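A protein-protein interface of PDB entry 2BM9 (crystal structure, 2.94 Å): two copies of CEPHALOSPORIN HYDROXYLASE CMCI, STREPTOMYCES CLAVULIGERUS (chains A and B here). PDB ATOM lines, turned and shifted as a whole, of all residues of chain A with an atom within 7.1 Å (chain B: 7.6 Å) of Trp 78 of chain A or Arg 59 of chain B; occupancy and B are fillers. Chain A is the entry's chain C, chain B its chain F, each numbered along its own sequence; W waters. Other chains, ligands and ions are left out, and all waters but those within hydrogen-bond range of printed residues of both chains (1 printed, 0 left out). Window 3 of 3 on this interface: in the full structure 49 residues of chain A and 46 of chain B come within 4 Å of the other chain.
A ring nitrogen (ND1) of His 74 of chain A lies close to the backbone carbonyl oxygen of Gln 57 of chain B, at 3.3 Å.
O of Ile 105 of chain A sits at hydrogen-bond distance from NE of Arg 59 of chain B (3.1 Å).
Position printed for both chains: 104.
Among the printed residues, no Asp or Glu carboxylate lies within 4 Å of a Lys or Arg side-chain nitrogen of the other chain.
NH2 of Arg 59 of chain B lies within salt-bridge range of OD2 of Asp 101 of chain B (3.1 Å).
The indole nitrogen (NE1) of Trp 58 of chain B sits at hydrogen-bond distance from the backbone carbonyl oxygen (O) of Ala 97 of chain B, 3.4 Å away.
NE1 of Trp 58 of chain B lies within hydrogen-bond range of OD2 of Asp 101 of chain B, 3.3 Å away.
N of Trp 78 of chain A lies within hydrogen-bond range of SD of Met 106 of chain A.
NH1 of Arg 81 of chain A sits at hydrogen-bond distance from O of Met 106 of chain A (3.4 Å).
The backbone NH (N) of Gly 60 of chain B is in hydrogen-bond range of the side-chain amide oxygen (OE1) of Gln 57 of chain B.
Of chain B, only Gln 57, Arg 59 and Gly 60 come within 4 Å of Trp 78 of chain A.
Arg 59 of chain B touches just these residues of chain A: His 74, Trp 78, Ile 105 and Met 106.
Of the printed residues of chain B, Met 106 of chain A touches Arg 59 (3.7 Å).
Of the printed residues of chain A, Gly 60 of chain B touches Trp 78 (3.6 Å).
Printed residues of chain A within 4 Å of Trp 58 of chain B: His 74, Leu 102 and Ile 105.
Of the printed residues of chain B, His 74 of chain A touches Gln 57 (3.1 Å), Trp 58 (3.3 Å) and Arg 59 (3.5 Å).
Leu 80 of chain A touches none of the printed residues of chain B.
Lys 104 of chain B touches none of the printed residues of chain A.
Among the printed residues, pairs that only touch across the chains: His 74 of chain A with Trp 58 of chain B (3.3 Å), Leu 102 of chain A with Trp 58 of chain B (3.3 Å), Trp 78 of chain A with Arg 59 of chain B (3.4 Å), His 74 of chain A with Arg 59 of chain B (3.5 Å), Asp 75 of chain A with Gln 57 of chain B (3.5 Å), Trp 78 of chain A with Gly 60 of chain B (3.6 Å), Trp 78 of chain A with Gln 57 of chain B (3.6 Å), Met 106 of chain A with Arg 59 of chain B (3.7 Å) and Ile 105 of chain A with Trp 58 of chain B (3.7 Å).
Water W1 lies within hydrogen-bond range of OD1 of Asp 75 of chain A and O of Gln 57 of chain B.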
ATOM      1  N   TYR A  73     -14.401   8.267 -15.526  1.00  0.00           N
ATOM      2  CA  TYR A  73     -15.129   9.337 -14.876  1.00  0.00           C
ATOM      3  C   TYR A  73     -14.138  10.265 -14.231  1.00  0.00           C
ATOM      4  O   TYR A  73     -14.397  11.457 -14.079  1.00  0.00           O
ATOM      5  CB  TYR A  73     -16.143   8.812 -13.867  1.00  0.00           C
ATOM      6  CG  TYR A  73     -17.518   8.624 -14.459  1.00  0.00           C
ATOM      7  CD1 TYR A  73     -18.190   7.424 -14.319  1.00  0.00           C
ATOM      8  CD2 TYR A  73     -18.153   9.653 -15.156  1.00  0.00           C
ATOM      9  CE1 TYR A  73     -19.445   7.240 -14.858  1.00  0.00           C
ATOM     10  CE2 TYR A  73     -19.419   9.474 -15.709  1.00  0.00           C
ATOM     11  CZ  TYR A  73     -20.058   8.263 -15.561  1.00  0.00           C
ATOM     12  OH  TYR A  73     -21.316   8.078 -16.098  1.00  0.00           O
ATOM     13  N   HIS A  74     -12.977   9.743 -13.879  1.00  0.00           N
ATOM     14  CA  HIS A  74     -11.978  10.627 -13.359  1.00  0.00           C
ATOM     15  C   HIS A  74     -11.591  11.545 -14.485  1.00  0.00           C
ATOM     16  O   HIS A  74     -11.942  12.700 -14.463  1.00  0.00           O
ATOM     17  CB  HIS A  74     -10.781   9.890 -12.828  1.00  0.00           C
ATOM     18  CG  HIS A  74      -9.596  10.770 -12.649  1.00  0.00           C
ATOM     19  ND1 HIS A  74      -8.420  10.319 -12.100  1.00  0.00           N
ATOM     20  CD2 HIS A  74      -9.398  12.076 -12.947  1.00  0.00           C
ATOM     21  CE1 HIS A  74      -7.546  11.309 -12.077  1.00  0.00           C
ATOM     22  NE2 HIS A  74      -8.114  12.385 -12.582  1.00  0.00           N
ATOM     23  N   ASP A  75     -10.901  11.028 -15.488  1.00  0.00           N
ATOM     24  CA  ASP A  75     -10.426  11.859 -16.606  1.00  0.00           C
ATOM     25  C   ASP A  75     -11.451  12.932 -16.982  1.00  0.00           C
ATOM     26  O   ASP A  75     -11.117  14.105 -17.043  1.00  0.00           O
ATOM     27  CB  ASP A  75     -10.077  10.996 -17.826  1.00  0.00           C
ATOM     28  CG  ASP A  75      -8.918  10.009 -17.552  1.00  0.00           C
ATOM     29  OD1 ASP A  75      -8.554   9.788 -16.370  1.00  0.00           O
ATOM     30  OD2 ASP A  75      -8.313   9.391 -18.454  1.00  0.00           O
ATOM     31  N   MET A  76     -12.702  12.527 -17.182  1.00  0.00           N
ATOM     32  CA  MET A  76     -13.805  13.454 -17.462  1.00  0.00           C
ATOM     33  C   MET A  76     -13.910  14.630 -16.473  1.00  0.00           C
ATOM     34  O   MET A  76     -13.916  15.776 -16.879  1.00  0.00           O
ATOM     35  CB  MET A  76     -15.158  12.710 -17.510  1.00  0.00           C
ATOM     36  CG  MET A  76     -16.174  13.366 -18.468  1.00  0.00           C
ATOM     37  SD  MET A  76     -17.906  12.795 -18.368  1.00  0.00           S
ATOM     38  CE  MET A  76     -17.736  11.138 -19.023  1.00  0.00           C
ATOM     39  N   LEU A  77     -14.035  14.340 -15.185  1.00  0.00           N
ATOM     40  CA  LEU A  77     -14.146  15.379 -14.153  1.00  0.00           C
ATOM     41  C   LEU A  77     -12.980  16.366 -14.201  1.00  0.00           C
ATOM     42  O   LEU A  77     -13.171  17.583 -14.215  1.00  0.00           O
ATOM     43  CB  LEU A  77     -14.221  14.739 -12.751  1.00  0.00           C
ATOM     44  CG  LEU A  77     -15.604  14.412 -12.168  1.00  0.00           C
ATOM     45  CD1 LEU A  77     -16.553  13.870 -13.243  1.00  0.00           C
ATOM     46  CD2 LEU A  77     -15.498  13.438 -10.978  1.00  0.00           C
ATOM     47  N   TRP A  78     -11.772  15.825 -14.227  1.00  0.00           N
ATOM     48  CA  TRP A  78     -10.559  16.623 -14.235  1.00  0.00           C
ATOM     49  C   TRP A  78     -10.484  17.547 -15.448  1.00  0.00           C
ATOM     50  O   TRP A  78      -9.858  18.584 -15.371  1.00  0.00           O
ATOM     51  CB  TRP A  78      -9.351  15.691 -14.179  1.00  0.00           C
ATOM     52  CG  TRP A  78      -8.060  16.351 -14.287  1.00  0.00           C
ATOM     53  CD1 TRP A  78      -7.259  16.409 -15.394  1.00  0.00           C
ATOM     54  CD2 TRP A  78      -7.375  17.060 -13.258  1.00  0.00           C
ATOM     55  NE1 TRP A  78      -6.115  17.121 -15.114  1.00  0.00           N
ATOM     56  CE2 TRP A  78      -6.162  17.534 -13.807  1.00  0.00           C
ATOM     57  CE3 TRP A  78      -7.663  17.354 -11.923  1.00  0.00           C
ATOM     58  CZ2 TRP A  78      -5.245  18.276 -13.070  1.00  0.00           C
ATOM     59  CZ3 TRP A  78      -6.748  18.102 -11.192  1.00  0.00           C
ATOM     60  CH2 TRP A  78      -5.555  18.549 -11.769  1.00  0.00           C
ATOM     61  N   GLU A  79     -11.127  17.180 -16.555  1.00  0.00           N
ATOM     62  CA  GLU A  79     -11.176  18.028 -17.758  1.00  0.00           C
ATOM     63  C   GLU A  79     -12.278  19.076 -17.688  1.00  0.00           C
ATOM     64  O   GLU A  79     -12.085  20.237 -18.085  1.00  0.00           O
ATOM     65  CB  GLU A  79     -11.395  17.197 -19.041  1.00  0.00           C
ATOM     66  CG  GLU A  79     -12.098  17.974 -20.164  1.00  0.00           C
ATOM     67  CD  GLU A  79     -12.215  17.207 -21.465  1.00  0.00           C
ATOM     68  OE1 GLU A  79     -13.016  16.243 -21.533  1.00  0.00           O
ATOM     69  OE2 GLU A  79     -11.519  17.591 -22.420  1.00  0.00           O
ATOM     70  N   LEU A  80     -13.445  18.651 -17.227  1.00  0.00           N
ATOM     71  CA  LEU A  80     -14.640  19.483 -17.266  1.00  0.00           C
ATOM     72  C   LEU A  80     -14.689  20.367 -16.038  1.00  0.00           C
ATOM     73  O   LEU A  80     -15.053  21.544 -16.130  1.00  0.00           O
ATOM     74  CB  LEU A  80     -15.905  18.613 -17.317  1.00  0.00           C
ATOM     75  CG  LEU A  80     -16.975  18.891 -18.378  1.00  0.00           C
ATOM     76  CD1 LEU A  80     -18.332  18.522 -17.813  1.00  0.00           C
ATOM     77  CD2 LEU A  80     -16.978  20.336 -18.881  1.00  0.00           C
ATOM     78  N   ARG A  81     -14.293  19.790 -14.904  1.00  0.00           N
ATOM     79  CA  ARG A  81     -14.472  20.404 -13.596  1.00  0.00           C
ATOM     80  C   ARG A  81     -15.947  20.757 -13.472  1.00  0.00           C
ATOM     81  O   ARG A  81     -16.329  21.921 -13.566  1.00  0.00           O
ATOM     82  CB  ARG A  81     -13.578  21.645 -13.415  1.00  0.00           C
ATOM     83  CG  ARG A  81     -12.086  21.336 -13.313  1.00  0.00           C
ATOM     84  CD  ARG A  81     -11.223  22.555 -13.084  1.00  0.00           C
ATOM     85  NE  ARG A  81     -11.273  23.006 -11.697  1.00  0.00           N
ATOM     86  CZ  ARG A  81     -10.648  22.413 -10.685  1.00  0.00           C
ATOM     87  NH1 ARG A  81      -9.910  21.320 -10.877  1.00  0.00           N
ATOM     88  NH2 ARG A  81     -10.768  22.918  -9.465  1.00  0.00           N
ATOM     89  N   PRO A  82     -16.779  19.736 -13.338  1.00  0.00           N
ATOM     90  CA  PRO A  82     -18.223  19.937 -13.250  1.00  0.00           C
ATOM     91  C   PRO A  82     -18.590  20.508 -11.915  1.00  0.00           C
ATOM     92  O   PRO A  82     -18.147  19.968 -10.916  1.00  0.00           O
ATOM     93  CB  PRO A  82     -18.782  18.526 -13.377  1.00  0.00           C
ATOM     94  CG  PRO A  82     -17.702  17.642 -12.936  1.00  0.00           C
ATOM     95  CD  PRO A  82     -16.419  18.312 -13.284  1.00  0.00           C
ATOM     96  N   LEU A 102     -14.368  12.725  -5.062  1.00  0.00           N
ATOM     97  CA  LEU A 102     -13.387  12.989  -6.109  1.00  0.00           C
ATOM     98  C   LEU A 102     -13.345  14.457  -6.579  1.00  0.00           C
ATOM     99  O   LEU A 102     -12.264  15.004  -6.776  1.00  0.00           O
ATOM    100  CB  LEU A 102     -13.624  12.063  -7.303  1.00  0.00           C
ATOM    101  CG  LEU A 102     -12.436  11.288  -7.894  1.00  0.00           C
ATOM    102  CD1 LEU A 102     -11.081  11.854  -7.471  1.00  0.00           C
ATOM    103  CD2 LEU A 102     -12.513   9.802  -7.568  1.00  0.00           C
ATOM    104  N   LYS A 104     -14.126  16.847  -4.714  1.00  0.00           N
ATOM    105  CA  LYS A 104     -13.626  17.536  -3.532  1.00  0.00           C
ATOM    106  C   LYS A 104     -12.106  17.647  -3.568  1.00  0.00           C
ATOM    107  O   LYS A 104     -11.548  18.730  -3.359  1.00  0.00           O
ATOM    108  CB  LYS A 104     -14.082  16.818  -2.251  1.00  0.00           C
ATOM    109  CG  LYS A 104     -13.440  17.326  -0.943  1.00  0.00           C
ATOM    110  CD  LYS A 104     -14.108  16.702   0.304  1.00  0.00           C
ATOM    111  CE  LYS A 104     -14.771  17.758   1.229  1.00  0.00           C
ATOM    112  NZ  LYS A 104     -15.941  17.205   2.007  1.00  0.00           N
ATOM    113  N   ILE A 105     -11.429  16.535  -3.840  1.00  0.00           N
ATOM    114  CA  ILE A 105      -9.960  16.532  -3.772  1.00  0.00           C
ATOM    115  C   ILE A 105      -9.320  17.099  -5.034  1.00  0.00           C
ATOM    116  O   ILE A 105      -8.208  17.617  -4.977  1.00  0.00           O
ATOM    117  CB  ILE A 105      -9.379  15.136  -3.396  1.00  0.00           C
ATOM    118  CG1 ILE A 105      -9.459  14.191  -4.581  1.00  0.00           C
ATOM    119  CG2 ILE A 105     -10.084  14.596  -2.140  1.00  0.00           C
ATOM    120  CD1 ILE A 105      -9.412  12.749  -4.187  1.00  0.00           C
ATOM    121  N   MET A 106     -10.039  17.023  -6.150  1.00  0.00           N
ATOM    122  CA  MET A 106      -9.686  17.768  -7.354  1.00  0.00           C
ATOM    123  C   MET A 106      -9.713  19.285  -7.119  1.00  0.00           C
ATOM    124  O   MET A 106      -9.100  20.047  -7.885  1.00  0.00           O
ATOM    125  CB  MET A 106     -10.640  17.423  -8.493  1.00  0.00           C
ATOM    126  CG  MET A 106     -10.451  16.032  -9.066  1.00  0.00           C
ATOM    127  SD  MET A 106     -11.329  15.805 -10.628  1.00  0.00           S
ATOM    128  CE  MET A 106     -10.860  14.144 -10.967  1.00  0.00           C
ATOM    129  N   GLY A 107     -10.411  19.715  -6.064  1.00  0.00           N
ATOM    130  CA  GLY A 107     -10.504  21.120  -5.703  1.00  0.00           C
ATOM    131  C   GLY A 107     -11.696  21.760  -6.375  1.00  0.00           C
ATOM    132  O   GLY A 107     -11.755  22.970  -6.523  1.00  0.00           O
ATOM    133  N   ILE A 108     -12.644  20.928  -6.793  1.00  0.00           N
ATOM    134  CA  ILE A 108     -13.864  21.382  -7.454  1.00  0.00           C
ATOM    135  C   ILE A 108     -15.025  21.507  -6.467  1.00  0.00           C
ATOM    136  O   ILE A 108     -15.207  20.680  -5.567  1.00  0.00           O
ATOM    137  CB  ILE A 108     -14.240  20.429  -8.614  1.00  0.00           C
ATOM    138  CG1 ILE A 108     -13.088  20.352  -9.615  1.00  0.00           C
ATOM    139  CG2 ILE A 108     -15.492  20.922  -9.338  1.00  0.00           C
ATOM    140  CD1 ILE A 108     -13.035  19.074 -10.378  1.00  0.00           C
ATOM    141  N   TYR A 217     -13.900   9.522 -24.363  1.00  0.00           N
ATOM    142  CA  TYR A 217     -14.328   8.699 -23.240  1.00  0.00           C
ATOM    143  C   TYR A 217     -15.275   7.548 -23.660  1.00  0.00           C
ATOM    144  O   TYR A 217     -15.259   6.461 -23.061  1.00  0.00           O
ATOM    145  CB  TYR A 217     -15.023   9.591 -22.218  1.00  0.00           C
ATOM    146  CG  TYR A 217     -14.196  10.785 -21.775  1.00  0.00           C
ATOM    147  CD1 TYR A 217     -14.664  12.075 -21.951  1.00  0.00           C
ATOM    148  CD2 TYR A 217     -12.952  10.615 -21.168  1.00  0.00           C
ATOM    149  CE1 TYR A 217     -13.917  13.160 -21.551  1.00  0.00           C
ATOM    150  CE2 TYR A 217     -12.199  11.700 -20.752  1.00  0.00           C
ATOM    151  CZ  TYR A 217     -12.683  12.968 -20.949  1.00  0.00           C
ATOM    152  OH  TYR A 217     -11.937  14.058 -20.548  1.00  0.00           O
ATOM    153  N   TYR B  24       2.041  14.209 -17.779  1.00  0.00           N
ATOM    154  CA  TYR B  24       0.837  13.693 -18.432  1.00  0.00           C
ATOM    155  C   TYR B  24       0.670  14.259 -19.842  1.00  0.00           C
ATOM    156  O   TYR B  24       0.941  15.431 -20.077  1.00  0.00           O
ATOM    157  CB  TYR B  24      -0.411  14.009 -17.616  1.00  0.00           C
ATOM    158  CG  TYR B  24      -1.686  13.479 -18.237  1.00  0.00           C
ATOM    159  CD1 TYR B  24      -1.970  12.104 -18.239  1.00  0.00           C
ATOM    160  CD2 TYR B  24      -2.604  14.339 -18.836  1.00  0.00           C
ATOM    161  CE1 TYR B  24      -3.147  11.601 -18.820  1.00  0.00           C
ATOM    162  CE2 TYR B  24      -3.781  13.848 -19.411  1.00  0.00           C
ATOM    163  CZ  TYR B  24      -4.043  12.481 -19.397  1.00  0.00           C
ATOM    164  OH  TYR B  24      -5.192  11.996 -19.963  1.00  0.00           O
ATOM    165  N   GLN B  57      -4.099   8.506 -15.400  1.00  0.00           N
ATOM    166  CA  GLN B  57      -3.694   9.741 -14.721  1.00  0.00           C
ATOM    167  C   GLN B  57      -4.410   9.957 -13.396  1.00  0.00           C
ATOM    168  O   GLN B  57      -5.393   9.292 -13.087  1.00  0.00           O
ATOM    169  CB  GLN B  57      -3.898  10.959 -15.635  1.00  0.00           C
ATOM    170  CG  GLN B  57      -5.342  11.160 -16.122  1.00  0.00           C
ATOM    171  CD  GLN B  57      -5.813  12.605 -16.101  1.00  0.00           C
ATOM    172  OE1 GLN B  57      -5.213  13.453 -15.448  1.00  0.00           O
ATOM    173  NE2 GLN B  57      -6.903  12.881 -16.813  1.00  0.00           N
ATOM    174  N   TRP B  58      -3.871  10.903 -12.633  1.00  0.00           N
ATOM    175  CA  TRP B  58      -4.344  11.248 -11.305  1.00  0.00           C
ATOM    176  C   TRP B  58      -4.020  12.716 -11.033  1.00  0.00           C
ATOM    177  O   TRP B  58      -2.922  13.050 -10.578  1.00  0.00           O
ATOM    178  CB  TRP B  58      -3.743  10.354 -10.221  1.00  0.00           C
ATOM    179  CG  TRP B  58      -4.269  10.727  -8.883  1.00  0.00           C
ATOM    180  CD1 TRP B  58      -3.573  11.279  -7.843  1.00  0.00           C
ATOM    181  CD2 TRP B  58      -5.621  10.636  -8.455  1.00  0.00           C
ATOM    182  NE1 TRP B  58      -4.415  11.520  -6.781  1.00  0.00           N
ATOM    183  CE2 TRP B  58      -5.681  11.133  -7.132  1.00  0.00           C
ATOM    184  CE3 TRP B  58      -6.798  10.176  -9.052  1.00  0.00           C
ATOM    185  CZ2 TRP B  58      -6.860  11.173  -6.403  1.00  0.00           C
ATOM    186  CZ3 TRP B  58      -7.964  10.216  -8.331  1.00  0.00           C
ATOM    187  CH2 TRP B  58      -7.990  10.711  -7.014  1.00  0.00           C
ATOM    188  N   ARG B  59      -4.987  13.579 -11.331  1.00  0.00           N
ATOM    189  CA  ARG B  59      -4.825  15.026 -11.223  1.00  0.00           C
ATOM    190  C   ARG B  59      -3.648  15.472 -12.043  1.00  0.00           C
ATOM    191  O   ARG B  59      -2.774  16.163 -11.548  1.00  0.00           O
ATOM    192  CB  ARG B  59      -4.630  15.464  -9.773  1.00  0.00           C
ATOM    193  CG  ARG B  59      -5.702  14.956  -8.839  1.00  0.00           C
ATOM    194  CD  ARG B  59      -6.517  16.041  -8.194  1.00  0.00           C
ATOM    195  NE  ARG B  59      -6.169  16.197  -6.790  1.00  0.00           N
ATOM    196  CZ  ARG B  59      -5.123  16.869  -6.337  1.00  0.00           C
ATOM    197  NH1 ARG B  59      -4.286  17.475  -7.170  1.00  0.00           N
ATOM    198  NH2 ARG B  59      -4.916  16.934  -5.028  1.00  0.00           N
ATOM    199  N   GLY B  60      -3.637  15.046 -13.297  1.00  0.00           N
ATOM    200  CA  GLY B  60      -2.567  15.358 -14.220  1.00  0.00           C
ATOM    201  C   GLY B  60      -1.215  14.759 -13.877  1.00  0.00           C
ATOM    202  O   GLY B  60      -0.193  15.307 -14.277  1.00  0.00           O
ATOM    203  N   LEU B  61      -1.200  13.643 -13.154  1.00  0.00           N
ATOM    204  CA  LEU B  61       0.037  12.941 -12.829  1.00  0.00           C
ATOM    205  C   LEU B  61      -0.081  11.482 -13.223  1.00  0.00           C
ATOM    206  O   LEU B  61      -0.994  10.795 -12.785  1.00  0.00           O
ATOM    207  CB  LEU B  61       0.322  13.043 -11.339  1.00  0.00           C
ATOM    208  CG  LEU B  61       0.371  14.472 -10.802  1.00  0.00           C
ATOM    209  CD1 LEU B  61       0.490  14.457  -9.289  1.00  0.00           C
ATOM    210  CD2 LEU B  61       1.528  15.257 -11.418  1.00  0.00           C
ATOM    211  N   ARG B  62       0.846  10.997 -14.034  1.00  0.00           N
ATOM    212  CA  ARG B  62       0.730   9.652 -14.588  1.00  0.00           C
ATOM    213  C   ARG B  62       0.719   8.545 -13.514  1.00  0.00           C
ATOM    214  O   ARG B  62       1.425   8.635 -12.506  1.00  0.00           O
ATOM    215  CB  ARG B  62       1.845   9.408 -15.611  1.00  0.00           C
ATOM    216  CG  ARG B  62       1.697  10.248 -16.884  1.00  0.00           C
ATOM    217  CD  ARG B  62       2.645   9.865 -18.032  1.00  0.00           C
ATOM    218  NE  ARG B  62       2.527   8.447 -18.390  1.00  0.00           N
ATOM    219  CZ  ARG B  62       3.546   7.594 -18.546  1.00  0.00           C
ATOM    220  NH1 ARG B  62       4.808   7.983 -18.389  1.00  0.00           N
ATOM    221  NH2 ARG B  62       3.290   6.330 -18.863  1.00  0.00           N
ATOM    222  N   MET B  63      -0.088   7.511 -13.758  1.00  0.00           N
ATOM    223  CA  MET B  63      -0.230   6.350 -12.880  1.00  0.00           C
ATOM    224  C   MET B  63       0.367   5.157 -13.574  1.00  0.00           C
ATOM    225  O   MET B  63       0.004   4.875 -14.709  1.00  0.00           O
ATOM    226  CB  MET B  63      -1.707   6.033 -12.636  1.00  0.00           C
ATOM    227  CG  MET B  63      -2.396   6.913 -11.630  1.00  0.00           C
ATOM    228  SD  MET B  63      -1.578   6.840 -10.032  1.00  0.00           S
ATOM    229  CE  MET B  63      -2.063   5.191  -9.450  1.00  0.00           C
ATOM    230  N   ALA B  97       1.219  10.431  -4.820  1.00  0.00           N
ATOM    231  CA  ALA B  97       0.165  11.429  -4.697  1.00  0.00           C
ATOM    232  C   ALA B  97      -1.195  10.771  -4.593  1.00  0.00           C
ATOM    233  O   ALA B  97      -2.159  11.411  -4.204  1.00  0.00           O
ATOM    234  CB  ALA B  97       0.187  12.364  -5.877  1.00  0.00           C
ATOM    235  N   ARG B 100      -1.402   9.255  -0.827  1.00  0.00           N
ATOM    236  CA  ARG B 100      -1.695  10.352   0.091  1.00  0.00           C
ATOM    237  C   ARG B 100      -3.140  10.730  -0.079  1.00  0.00           C
ATOM    238  O   ARG B 100      -3.892  10.743   0.885  1.00  0.00           O
ATOM    239  CB  ARG B 100      -0.825  11.593  -0.161  1.00  0.00           C
ATOM    240  CG  ARG B 100      -1.588  12.951  -0.143  1.00  0.00           C
ATOM    241  CD  ARG B 100      -0.693  14.162  -0.023  1.00  0.00           C
ATOM    242  NE  ARG B 100      -1.043  15.284  -0.904  1.00  0.00           N
ATOM    243  CZ  ARG B 100      -0.928  15.293  -2.234  1.00  0.00           C
ATOM    244  NH1 ARG B 100      -0.486  14.227  -2.882  1.00  0.00           N
ATOM    245  NH2 ARG B 100      -1.257  16.380  -2.927  1.00  0.00           N
ATOM    246  N   ASP B 101      -3.534  11.038  -1.308  1.00  0.00           N
ATOM    247  CA  ASP B 101      -4.851  11.607  -1.528  1.00  0.00           C
ATOM    248  C   ASP B 101      -5.923  10.622  -1.073  1.00  0.00           C
ATOM    249  O   ASP B 101      -7.027  11.033  -0.726  1.00  0.00           O
ATOM    250  CB  ASP B 101      -5.056  12.020  -2.996  1.00  0.00           C
ATOM    251  CG  ASP B 101      -4.434  13.400  -3.331  1.00  0.00           C
ATOM    252  OD1 ASP B 101      -3.891  14.092  -2.421  1.00  0.00           O
ATOM    253  OD2 ASP B 101      -4.443  13.876  -4.497  1.00  0.00           O
ATOM    254  N   LYS B 104      -6.113  10.104   2.952  1.00  0.00           N
ATOM    255  CA  LYS B 104      -6.697  11.362   3.429  1.00  0.00           C
ATOM    256  C   LYS B 104      -8.211  11.230   3.543  1.00  0.00           C
ATOM    257  O   LYS B 104      -8.759  11.422   4.616  1.00  0.00           O
ATOM    258  CB  LYS B 104      -6.346  12.533   2.490  1.00  0.00           C
ATOM    259  CG  LYS B 104      -5.776  13.768   3.174  1.00  0.00           C
ATOM    260  CD  LYS B 104      -6.105  15.026   2.375  1.00  0.00           C
ATOM    261  CE  LYS B 104      -5.009  16.067   2.479  1.00  0.00           C
ATOM    262  NZ  LYS B 104      -4.624  16.346   3.885  1.00  0.00           N
ATOM    263  N   GLN B 123       7.230  14.604 -11.024  1.00  0.00           N
ATOM    264  CA  GLN B 123       6.485  15.719 -11.622  1.00  0.00           C
ATOM    265  C   GLN B 123       5.384  16.307 -10.696  1.00  0.00           C
ATOM    266  O   GLN B 123       4.546  17.107 -11.141  1.00  0.00           O
ATOM    267  CB  GLN B 123       5.894  15.269 -12.970  1.00  0.00           C
ATOM    268  CG  GLN B 123       6.665  15.767 -14.201  1.00  0.00           C
ATOM    269  CD  GLN B 123       5.934  16.868 -14.972  1.00  0.00           C
ATOM    270  OE1 GLN B 123       4.772  17.182 -14.691  1.00  0.00           O
ATOM    271  NE2 GLN B 123       6.617  17.453 -15.945  1.00  0.00           N
ATOM    272  N   PRO B 125       3.859  18.842  -8.156  1.00  0.00           N
ATOM    273  CA  PRO B 125       4.064  20.232  -7.738  1.00  0.00           C
ATOM    274  C   PRO B 125       4.817  20.315  -6.417  1.00  0.00           C
ATOM    275  O   PRO B 125       4.520  19.564  -5.493  1.00  0.00           O
ATOM    276  CB  PRO B 125       2.638  20.761  -7.562  1.00  0.00           C
ATOM    277  CG  PRO B 125       1.801  19.935  -8.475  1.00  0.00           C
ATOM    278  CD  PRO B 125       2.476  18.591  -8.604  1.00  0.00           C
ATOM    279  N   ASP B 128       2.306  20.395  -3.197  1.00  0.00           N
ATOM    280  CA  ASP B 128       1.232  19.411  -3.041  1.00  0.00           C
ATOM    281  C   ASP B 128       1.700  18.262  -2.131  1.00  0.00           C
ATOM    282  O   ASP B 128       1.048  17.219  -2.046  1.00  0.00           O
ATOM    283  CB  ASP B 128       0.834  18.853  -4.420  1.00  0.00           C
ATOM    284  CG  ASP B 128      -0.418  19.514  -4.991  1.00  0.00           C
ATOM    285  OD1 ASP B 128      -1.343  18.767  -5.417  1.00  0.00           O
ATOM    286  OD2 ASP B 128      -0.543  20.762  -5.067  1.00  0.00           O
HETATM  287  O   HOH W   1      -7.097   7.888 -15.027  1.00  0.00           O
